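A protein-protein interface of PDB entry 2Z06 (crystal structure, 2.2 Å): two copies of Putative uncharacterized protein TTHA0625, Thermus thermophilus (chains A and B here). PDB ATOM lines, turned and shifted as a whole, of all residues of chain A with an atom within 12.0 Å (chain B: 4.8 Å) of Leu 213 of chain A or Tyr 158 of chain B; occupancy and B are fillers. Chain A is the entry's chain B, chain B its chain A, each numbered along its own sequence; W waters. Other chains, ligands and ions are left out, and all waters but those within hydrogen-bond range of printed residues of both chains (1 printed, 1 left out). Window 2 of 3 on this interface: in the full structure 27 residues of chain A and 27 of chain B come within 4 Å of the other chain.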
ATOM      1  N   SER A 199      14.459 -12.487  21.562  1.00  0.00           N
ATOM      2  CA  SER A 199      15.024 -13.465  22.475  1.00  0.00           C
ATOM      3  C   SER A 199      14.172 -14.725  22.458  1.00  0.00           C
ATOM      4  O   SER A 199      13.290 -14.888  21.619  1.00  0.00           O
ATOM      5  CB  SER A 199      14.987 -12.905  23.894  1.00  0.00           C
ATOM      6  OG  SER A 199      13.630 -12.699  24.289  1.00  0.00           O
ATOM      7  N   ILE A 200      14.446 -15.604  23.415  1.00  0.00           N
ATOM      8  CA  ILE A 200      13.698 -16.835  23.587  1.00  0.00           C
ATOM      9  C   ILE A 200      13.209 -16.770  25.032  1.00  0.00           C
ATOM     10  O   ILE A 200      13.969 -17.019  25.973  1.00  0.00           O
ATOM     11  CB  ILE A 200      14.588 -18.080  23.375  1.00  0.00           C
ATOM     12  CG1 ILE A 200      14.914 -18.235  21.890  1.00  0.00           C
ATOM     13  CG2 ILE A 200      13.882 -19.326  23.902  1.00  0.00           C
ATOM     14  CD1 ILE A 200      15.756 -19.445  21.587  1.00  0.00           C
ATOM     15  N   GLU A 204      18.737 -14.729  26.136  1.00  0.00           N
ATOM     16  CA  GLU A 204      19.464 -14.536  24.879  1.00  0.00           C
ATOM     17  C   GLU A 204      19.319 -15.780  24.005  1.00  0.00           C
ATOM     18  O   GLU A 204      19.476 -16.908  24.476  1.00  0.00           O
ATOM     19  CB  GLU A 204      20.949 -14.255  25.152  1.00  0.00           C
ATOM     20  CG  GLU A 204      21.269 -12.796  25.412  1.00  0.00           C
ATOM     21  CD  GLU A 204      22.676 -12.606  25.937  1.00  0.00           C
ATOM     22  OE1 GLU A 204      23.568 -13.392  25.537  1.00  0.00           O
ATOM     23  OE2 GLU A 204      22.890 -11.666  26.740  1.00  0.00           O
ATOM     24  N   VAL A 205      19.014 -15.560  22.733  1.00  0.00           N
ATOM     25  CA  VAL A 205      18.819 -16.649  21.785  1.00  0.00           C
ATOM     26  C   VAL A 205      19.892 -17.729  21.835  1.00  0.00           C
ATOM     27  O   VAL A 205      19.606 -18.875  22.188  1.00  0.00           O
ATOM     28  CB  VAL A 205      18.718 -16.105  20.344  1.00  0.00           C
ATOM     29  CG1 VAL A 205      18.523 -17.249  19.357  1.00  0.00           C
ATOM     30  CG2 VAL A 205      17.559 -15.125  20.249  1.00  0.00           C
ATOM     31  N   GLU A 206      21.125 -17.368  21.495  1.00  0.00           N
ATOM     32  CA  GLU A 206      22.213 -18.340  21.480  1.00  0.00           C
ATOM     33  C   GLU A 206      22.391 -19.120  22.769  1.00  0.00           C
ATOM     34  O   GLU A 206      22.865 -20.257  22.738  1.00  0.00           O
ATOM     35  CB  GLU A 206      23.530 -17.670  21.074  1.00  0.00           C
ATOM     36  CG  GLU A 206      23.877 -17.868  19.588  1.00  0.00           C
ATOM     37  CD  GLU A 206      24.308 -19.304  19.256  1.00  0.00           C
ATOM     38  OE1 GLU A 206      24.588 -19.596  18.066  1.00  0.00           O
ATOM     39  OE2 GLU A 206      24.373 -20.138  20.189  1.00  0.00           O
ATOM     40  N   THR A 207      22.005 -18.528  23.898  1.00  0.00           N
ATOM     41  CA  THR A 207      22.114 -19.217  25.178  1.00  0.00           C
ATOM     42  C   THR A 207      21.153 -20.403  25.204  1.00  0.00           C
ATOM     43  O   THR A 207      21.547 -21.530  25.509  1.00  0.00           O
ATOM     44  CB  THR A 207      21.778 -18.274  26.354  1.00  0.00           C
ATOM     45  OG1 THR A 207      22.829 -17.313  26.509  1.00  0.00           O
ATOM     46  CG2 THR A 207      21.598 -19.067  27.657  1.00  0.00           C
ATOM     47  N   PHE A 208      19.892 -20.142  24.879  1.00  0.00           N
ATOM     48  CA  PHE A 208      18.877 -21.187  24.859  1.00  0.00           C
ATOM     49  C   PHE A 208      19.161 -22.175  23.747  1.00  0.00           C
ATOM     50  O   PHE A 208      18.936 -23.376  23.890  1.00  0.00           O
ATOM     51  CB  PHE A 208      17.488 -20.580  24.652  1.00  0.00           C
ATOM     52  CG  PHE A 208      16.676 -20.514  25.901  1.00  0.00           C
ATOM     53  CD1 PHE A 208      16.187 -21.678  26.483  1.00  0.00           C
ATOM     54  CD2 PHE A 208      16.451 -19.303  26.533  1.00  0.00           C
ATOM     55  CE1 PHE A 208      15.487 -21.641  27.681  1.00  0.00           C
ATOM     56  CE2 PHE A 208      15.751 -19.251  27.738  1.00  0.00           C
ATOM     57  CZ  PHE A 208      15.269 -20.427  28.312  1.00  0.00           C
ATOM     58  N   LEU A 209      19.663 -21.656  22.638  1.00  0.00           N
ATOM     59  CA  LEU A 209      19.972 -22.480  21.492  1.00  0.00           C
ATOM     60  C   LEU A 209      21.057 -23.458  21.899  1.00  0.00           C
ATOM     61  O   LEU A 209      20.982 -24.654  21.602  1.00  0.00           O
ATOM     62  CB  LEU A 209      20.437 -21.590  20.343  1.00  0.00           C
ATOM     63  CG  LEU A 209      20.380 -22.122  18.912  1.00  0.00           C
ATOM     64  CD1 LEU A 209      19.418 -23.303  18.805  1.00  0.00           C
ATOM     65  CD2 LEU A 209      19.936 -20.978  18.001  1.00  0.00           C
ATOM     66  N   ALA A 210      22.061 -22.947  22.600  1.00  0.00           N
ATOM     67  CA  ALA A 210      23.157 -23.782  23.056  1.00  0.00           C
ATOM     68  C   ALA A 210      22.649 -24.867  24.007  1.00  0.00           C
ATOM     69  O   ALA A 210      23.209 -25.958  24.060  1.00  0.00           O
ATOM     70  CB  ALA A 210      24.216 -22.924  23.746  1.00  0.00           C
ATOM     71  N   ARG A 211      21.597 -24.570  24.763  1.00  0.00           N
ATOM     72  CA  ARG A 211      21.041 -25.570  25.678  1.00  0.00           C
ATOM     73  C   ARG A 211      20.423 -26.724  24.901  1.00  0.00           C
ATOM     74  O   ARG A 211      20.717 -27.892  25.159  1.00  0.00           O
ATOM     75  CB  ARG A 211      19.964 -24.968  26.572  1.00  0.00           C
ATOM     76  CG  ARG A 211      20.467 -23.955  27.566  1.00  0.00           C
ATOM     77  CD  ARG A 211      19.324 -23.435  28.418  1.00  0.00           C
ATOM     78  NE  ARG A 211      19.787 -22.431  29.358  1.00  0.00           N
ATOM     79  CZ  ARG A 211      19.005 -21.792  30.217  1.00  0.00           C
ATOM     80  NH1 ARG A 211      17.703 -22.057  30.258  1.00  0.00           N
ATOM     81  NH2 ARG A 211      19.527 -20.884  31.031  1.00  0.00           N
ATOM     82  N   PHE A 212      19.564 -26.400  23.945  1.00  0.00           N
ATOM     83  CA  PHE A 212      18.924 -27.451  23.171  1.00  0.00           C
ATOM     84  C   PHE A 212      19.889 -28.240  22.313  1.00  0.00           C
ATOM     85  O   PHE A 212      19.706 -29.438  22.139  1.00  0.00           O
ATOM     86  CB  PHE A 212      17.809 -26.881  22.292  1.00  0.00           C
ATOM     87  CG  PHE A 212      16.618 -26.439  23.068  1.00  0.00           C
ATOM     88  CD1 PHE A 212      16.494 -25.114  23.487  1.00  0.00           C
ATOM     89  CD2 PHE A 212      15.648 -27.359  23.450  1.00  0.00           C
ATOM     90  CE1 PHE A 212      15.426 -24.717  24.275  1.00  0.00           C
ATOM     91  CE2 PHE A 212      14.575 -26.970  24.239  1.00  0.00           C
ATOM     92  CZ  PHE A 212      14.463 -25.646  24.654  1.00  0.00           C
ATOM     93  N   LEU A 213      20.925 -27.578  21.807  1.00  0.00           N
ATOM     94  CA  LEU A 213      21.910 -28.223  20.943  1.00  0.00           C
ATOM     95  C   LEU A 213      22.932 -29.122  21.625  1.00  0.00           C
ATOM     96  O   LEU A 213      23.174 -30.240  21.174  1.00  0.00           O
ATOM     97  CB  LEU A 213      22.653 -27.168  20.133  1.00  0.00           C
ATOM     98  CG  LEU A 213      21.791 -26.383  19.148  1.00  0.00           C
ATOM     99  CD1 LEU A 213      22.635 -25.295  18.498  1.00  0.00           C
ATOM    100  CD2 LEU A 213      21.211 -27.337  18.104  1.00  0.00           C
ATOM    101  N   THR A 214      23.531 -28.632  22.707  1.00  0.00           N
ATOM    102  CA  THR A 214      24.549 -29.388  23.422  1.00  0.00           C
ATOM    103  C   THR A 214      23.987 -30.306  24.493  1.00  0.00           C
ATOM    104  O   THR A 214      24.594 -31.319  24.836  1.00  0.00           O
ATOM    105  CB  THR A 214      25.577 -28.433  24.085  1.00  0.00           C
ATOM    106  OG1 THR A 214      24.987 -27.789  25.220  1.00  0.00           O
ATOM    107  CG2 THR A 214      26.006 -27.356  23.098  1.00  0.00           C
ATOM    108  N   GLY A 215      22.819 -29.958  25.022  1.00  0.00           N
ATOM    109  CA  GLY A 215      22.232 -30.767  26.070  1.00  0.00           C
ATOM    110  C   GLY A 215      22.999 -30.515  27.357  1.00  0.00           C
ATOM    111  O   GLY A 215      22.876 -31.257  28.323  1.00  0.00           O
ATOM    112  N   ARG A 216      23.800 -29.455  27.367  1.00  0.00           N
ATOM    113  CA  ARG A 216      24.590 -29.107  28.538  1.00  0.00           C
ATOM    114  C   ARG A 216      24.122 -27.798  29.147  1.00  0.00           C
ATOM    115  O   ARG A 216      23.735 -26.871  28.436  1.00  0.00           O
ATOM    116  CB  ARG A 216      26.070 -29.011  28.168  1.00  0.00           C
ATOM    117  CG  ARG A 216      26.745 -30.365  28.018  1.00  0.00           C
ATOM    118  CD  ARG A 216      27.844 -30.301  26.975  1.00  0.00           C
ATOM    119  NE  ARG A 216      28.774 -29.218  27.255  1.00  0.00           N
ATOM    120  CZ  ARG A 216      29.433 -28.553  26.319  1.00  0.00           C
ATOM    121  NH1 ARG A 216      29.262 -28.865  25.042  1.00  0.00           N
ATOM    122  NH2 ARG A 216      30.252 -27.570  26.661  1.00  0.00           N
ATOM    123  N   PRO A 217      24.161 -27.703  30.483  1.00  0.00           N
ATOM    124  CA  PRO A 217      23.734 -26.494  31.198  1.00  0.00           C
ATOM    125  C   PRO A 217      24.355 -25.211  30.659  1.00  0.00           C
ATOM    126  O   PRO A 217      25.548 -25.158  30.374  1.00  0.00           O
ATOM    127  CB  PRO A 217      24.142 -26.785  32.641  1.00  0.00           C
ATOM    128  CG  PRO A 217      25.331 -27.709  32.476  1.00  0.00           C
ATOM    129  CD  PRO A 217      24.842 -28.637  31.395  1.00  0.00           C
ATOM    130  N   GLN A 218      23.524 -24.186  30.513  1.00  0.00           N
ATOM    131  CA  GLN A 218      23.955 -22.883  30.024  1.00  0.00           C
ATOM    132  C   GLN A 218      23.300 -21.847  30.947  1.00  0.00           C
ATOM    133  O   GLN A 218      22.075 -21.696  30.960  1.00  0.00           O
ATOM    134  CB  GLN A 218      23.490 -22.680  28.578  1.00  0.00           C
ATOM    135  CG  GLN A 218      23.769 -23.864  27.652  1.00  0.00           C
ATOM    136  CD  GLN A 218      25.215 -23.934  27.157  1.00  0.00           C
ATOM    137  OE1 GLN A 218      25.683 -24.994  26.725  1.00  0.00           O
ATOM    138  NE2 GLN A 218      25.917 -22.806  27.198  1.00  0.00           N
ATOM    139  N   ASP B 123      16.992 -36.021  18.151  1.00  0.00           N
ATOM    140  CA  ASP B 123      17.246 -34.593  18.125  1.00  0.00           C
ATOM    141  C   ASP B 123      16.613 -33.960  16.871  1.00  0.00           C
ATOM    142  O   ASP B 123      17.062 -34.191  15.749  1.00  0.00           O
ATOM    143  CB  ASP B 123      18.772 -34.387  18.158  1.00  0.00           C
ATOM    144  CG  ASP B 123      19.176 -32.947  18.050  1.00  0.00           C
ATOM    145  OD1 ASP B 123      20.347 -32.648  18.349  1.00  0.00           O
ATOM    146  OD2 ASP B 123      18.340 -32.113  17.654  1.00  0.00           O
ATOM    147  N   PHE B 125      16.645 -30.812  15.986  1.00  0.00           N
ATOM    148  CA  PHE B 125      17.517 -29.819  15.371  1.00  0.00           C
ATOM    149  C   PHE B 125      18.413 -30.478  14.321  1.00  0.00           C
ATOM    150  O   PHE B 125      18.439 -30.061  13.164  1.00  0.00           O
ATOM    151  CB  PHE B 125      18.384 -29.119  16.423  1.00  0.00           C
ATOM    152  CG  PHE B 125      17.601 -28.318  17.423  1.00  0.00           C
ATOM    153  CD1 PHE B 125      16.975 -28.942  18.494  1.00  0.00           C
ATOM    154  CD2 PHE B 125      17.497 -26.932  17.296  1.00  0.00           C
ATOM    155  CE1 PHE B 125      16.258 -28.201  19.429  1.00  0.00           C
ATOM    156  CE2 PHE B 125      16.778 -26.175  18.230  1.00  0.00           C
ATOM    157  CZ  PHE B 125      16.158 -26.816  19.300  1.00  0.00           C
ATOM    158  N   ARG B 126      19.145 -31.511  14.714  1.00  0.00           N
ATOM    159  CA  ARG B 126      20.023 -32.173  13.763  1.00  0.00           C
ATOM    160  C   ARG B 126      19.241 -33.073  12.801  1.00  0.00           C
ATOM    161  O   ARG B 126      19.732 -33.434  11.731  1.00  0.00           O
ATOM    162  CB  ARG B 126      21.101 -32.950  14.520  1.00  0.00           C
ATOM    163  CG  ARG B 126      21.972 -32.014  15.361  1.00  0.00           C
ATOM    164  CD  ARG B 126      23.134 -32.725  16.005  1.00  0.00           C
ATOM    165  NE  ARG B 126      24.066 -31.776  16.604  1.00  0.00           N
ATOM    166  CZ  ARG B 126      23.863 -31.134  17.748  1.00  0.00           C
ATOM    167  NH1 ARG B 126      22.751 -31.336  18.443  1.00  0.00           N
ATOM    168  NH2 ARG B 126      24.779 -30.286  18.198  1.00  0.00           N
ATOM    169  N   ASP B 129      18.638 -30.774  10.042  1.00  0.00           N
ATOM    170  CA  ASP B 129      19.866 -30.497   9.305  1.00  0.00           C
ATOM    171  C   ASP B 129      20.106 -31.541   8.223  1.00  0.00           C
ATOM    172  O   ASP B 129      20.374 -31.197   7.075  1.00  0.00           O
ATOM    173  CB  ASP B 129      21.084 -30.460  10.244  1.00  0.00           C
ATOM    174  CG  ASP B 129      21.052 -29.284  11.211  1.00  0.00           C
ATOM    175  OD1 ASP B 129      20.772 -28.148  10.773  1.00  0.00           O
ATOM    176  OD2 ASP B 129      21.320 -29.496  12.413  1.00  0.00           O
ATOM    177  N   ALA B 154      13.435 -22.027  19.904  1.00  0.00           N
ATOM    178  CA  ALA B 154      14.806 -22.436  19.628  1.00  0.00           C
ATOM    179  C   ALA B 154      14.855 -23.042  18.223  1.00  0.00           C
ATOM    180  O   ALA B 154      15.744 -22.715  17.426  1.00  0.00           O
ATOM    181  CB  ALA B 154      15.277 -23.452  20.661  1.00  0.00           C
ATOM    182  N   LEU B 155      13.896 -23.917  17.918  1.00  0.00           N
ATOM    183  CA  LEU B 155      13.842 -24.531  16.596  1.00  0.00           C
ATOM    184  C   LEU B 155      13.656 -23.489  15.489  1.00  0.00           C
ATOM    185  O   LEU B 155      14.283 -23.585  14.438  1.00  0.00           O
ATOM    186  CB  LEU B 155      12.726 -25.584  16.536  1.00  0.00           C
ATOM    187  CG  LEU B 155      13.130 -26.938  17.143  1.00  0.00           C
ATOM    188  CD1 LEU B 155      11.907 -27.799  17.456  1.00  0.00           C
ATOM    189  CD2 LEU B 155      14.069 -27.647  16.177  1.00  0.00           C
ATOM    190  N   ALA B 156      12.814 -22.486  15.728  1.00  0.00           N
ATOM    191  CA  ALA B 156      12.574 -21.448  14.727  1.00  0.00           C
ATOM    192  C   ALA B 156      13.862 -20.679  14.437  1.00  0.00           C
ATOM    193  O   ALA B 156      14.268 -20.532  13.282  1.00  0.00           O
ATOM    194  CB  ALA B 156      11.494 -20.491  15.202  1.00  0.00           C
ATOM    195  N   HIS B 157      14.504 -20.179  15.485  1.00  0.00           N
ATOM    196  CA  HIS B 157      15.745 -19.446  15.298  1.00  0.00           C
ATOM    197  C   HIS B 157      16.775 -20.315  14.582  1.00  0.00           C
ATOM    198  O   HIS B 157      17.432 -19.860  13.649  1.00  0.00           O
ATOM    199  CB  HIS B 157      16.281 -18.961  16.650  1.00  0.00           C
ATOM    200  CG  HIS B 157      15.528 -17.790  17.198  1.00  0.00           C
ATOM    201  ND1 HIS B 157      15.613 -16.530  16.645  1.00  0.00           N
ATOM    202  CD2 HIS B 157      14.616 -17.700  18.195  1.00  0.00           C
ATOM    203  CE1 HIS B 157      14.784 -15.717  17.273  1.00  0.00           C
ATOM    204  NE2 HIS B 157      14.166 -16.402  18.219  1.00  0.00           N
ATOM    205  N   TYR B 158      16.892 -21.570  15.008  1.00  0.00           N
ATOM    206  CA  TYR B 158      17.842 -22.507  14.414  1.00  0.00           C
ATOM    207  C   TYR B 158      17.598 -22.722  12.921  1.00  0.00           C
ATOM    208  O   TYR B 158      18.525 -23.024  12.171  1.00  0.00           O
ATOM    209  CB  TYR B 158      17.766 -23.853  15.135  1.00  0.00           C
ATOM    210  CG  TYR B 158      18.883 -24.807  14.778  1.00  0.00           C
ATOM    211  CD1 TYR B 158      20.176 -24.609  15.271  1.00  0.00           C
ATOM    212  CD2 TYR B 158      18.653 -25.905  13.946  1.00  0.00           C
ATOM    213  CE1 TYR B 158      21.211 -25.483  14.945  1.00  0.00           C
ATOM    214  CE2 TYR B 158      19.682 -26.789  13.614  1.00  0.00           C
ATOM    215  CZ  TYR B 158      20.959 -26.569  14.118  1.00  0.00           C
ATOM    216  OH  TYR B 158      21.982 -27.424  13.796  1.00  0.00           O
ATOM    217  N   LEU B 159      16.349 -22.570  12.494  1.00  0.00           N
ATOM    218  CA  LEU B 159      15.996 -22.749  11.088  1.00  0.00           C
ATOM    219  C   LEU B 159      15.906 -21.417  10.356  1.00  0.00           C
ATOM    220  O   LEU B 159      15.690 -21.383   9.145  1.00  0.00           O
ATOM    221  CB  LEU B 159      14.641 -23.455  10.967  1.00  0.00           C
ATOM    222  CG  LEU B 159      14.515 -24.941  11.308  1.00  0.00           C
ATOM    223  CD1 LEU B 159      13.056 -25.272  11.602  1.00  0.00           C
ATOM    224  CD2 LEU B 159      15.041 -25.789  10.151  1.00  0.00           C
ATOM    225  N   ASP B 160      16.054 -20.321  11.091  1.00  0.00           N
ATOM    226  CA  ASP B 160      15.946 -18.990  10.508  1.00  0.00           C
ATOM    227  C   ASP B 160      16.850 -18.825   9.285  1.00  0.00           C
ATOM    228  O   ASP B 160      18.042 -19.118   9.335  1.00  0.00           O
ATOM    229  CB  ASP B 160      16.263 -17.941  11.580  1.00  0.00           C
ATOM    230  CG  ASP B 160      15.946 -16.519  11.135  1.00  0.00           C
ATOM    231  OD1 ASP B 160      15.107 -16.343  10.222  1.00  0.00           O
ATOM    232  OD2 ASP B 160      16.527 -15.570  11.720  1.00  0.00           O
ATOM    233  N   ARG B 162      16.743 -20.562   6.680  1.00  0.00           N
ATOM    234  CA  ARG B 162      16.700 -21.825   5.955  1.00  0.00           C
ATOM    235  C   ARG B 162      15.245 -22.176   5.630  1.00  0.00           C
ATOM    236  O   ARG B 162      14.904 -22.466   4.489  1.00  0.00           O
ATOM    237  CB  ARG B 162      17.345 -22.934   6.786  1.00  0.00           C
ATOM    238  CG  ARG B 162      18.841 -22.764   6.955  1.00  0.00           C
ATOM    239  CD  ARG B 162      19.495 -24.062   7.377  1.00  0.00           C
ATOM    240  NE  ARG B 162      19.332 -24.339   8.798  1.00  0.00           N
ATOM    241  CZ  ARG B 162      19.584 -25.519   9.351  1.00  0.00           C
ATOM    242  NH1 ARG B 162      20.000 -26.528   8.595  1.00  0.00           N
ATOM    243  NH2 ARG B 162      19.442 -25.686  10.660  1.00  0.00           N
HETATM  244  O   HOH W   1      11.791 -15.962  19.912  1.00  0.00           O
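Of the 17 printed residues of chain A, 6 touch a printed residue of chain B. Printed residues of chain A that touch a printed residue of chain B: Ser 199, Ile 200, Val 205, Leu 209, Phe 212 and Leu 213.
NH1 of Arg 126 of chain B lies within hydrogen-bond range of O of Leu 213 of chain A, at 3.0 Å.
Water W1 bridges O of Ser 199 of chain A (2.5 Å) and NE2 of His 157 of chain B (2.9 Å).
Leu 213 of chain A touches three residues of chain B. Of chain A, only Leu 209 and Leu 213 come within 4 Å of Tyr 158 of chain B. No residue of chain A comes within 4 Å of Asp 129 of chain B. No residue of chain A comes within 4 Å of Ala 156 of chain B. His 157 of chain B touches three residues of chain A. No residue of chain A comes within 4 Å of Asp 160 of chain B. Of the printed residues of chain B, Ser 199 of chain A touches His 157 (3.8 Å). Printed residues of chain B within 4 Å of Ile 200 of chain A: Ala 154 (3.7 Å) and His 157 (3.7 Å). Of the printed residues of chain B, Leu 209 of chain A touches Phe 125 (3.9 Å), Ala 154 (3.97 Å) and Tyr 158 (3.8 Å). The nearest residue of chain A that does not touch Tyr 158 of chain B is Val 205 of chain A (6.3 Å).
Ser 199 of chain A touches His 157 of chain B. CA of Ala 154 of chain B touches CD1 of Ile 200 of chain A, 3.7 Å away. Ile 200 of chain A touches His 157 of chain B. His 157 of chain B touches Val 205 of chain A (CG to CG1, 3.7 Å). Phe 125 of chain B touches Leu 209 of chain A. Leu 209 of chain A touches Ala 154 of chain B. Phe 212 of chain A touches Phe 125 of chain B (CB to CZ, 3.4 Å). Phe 212 of chain A touches Ala 154 of chain B (CD1 to CB, 3.5 Å). Phe 125 of chain B touches Leu 213 of chain A. CE1 of Tyr 158 of chain B touches CD2 of Leu 213 of chain A, at 3.7 Å.
The backbone NH of Phe 125 of chain B is in hydrogen-bond range of the side-chain carboxylate of Asp 123 of chain B (2.7 Å). The side-chain carboxylate of Asp 123 of chain B is in salt-bridge range of the guanidinium group of Arg 126 of chain B, at 2.7 Å. OD2 of Asp 129 of chain B sits at hydrogen-bond distance from OH of Tyr 158 of chain B (2.6 Å). NH2 of Arg 162 of chain B lies close to O of Tyr 158 of chain B.
No position is printed for both chains. Of the 12 pairs that touch across the chains among the printed residues, none has its exchanged pair printed and touching as well.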
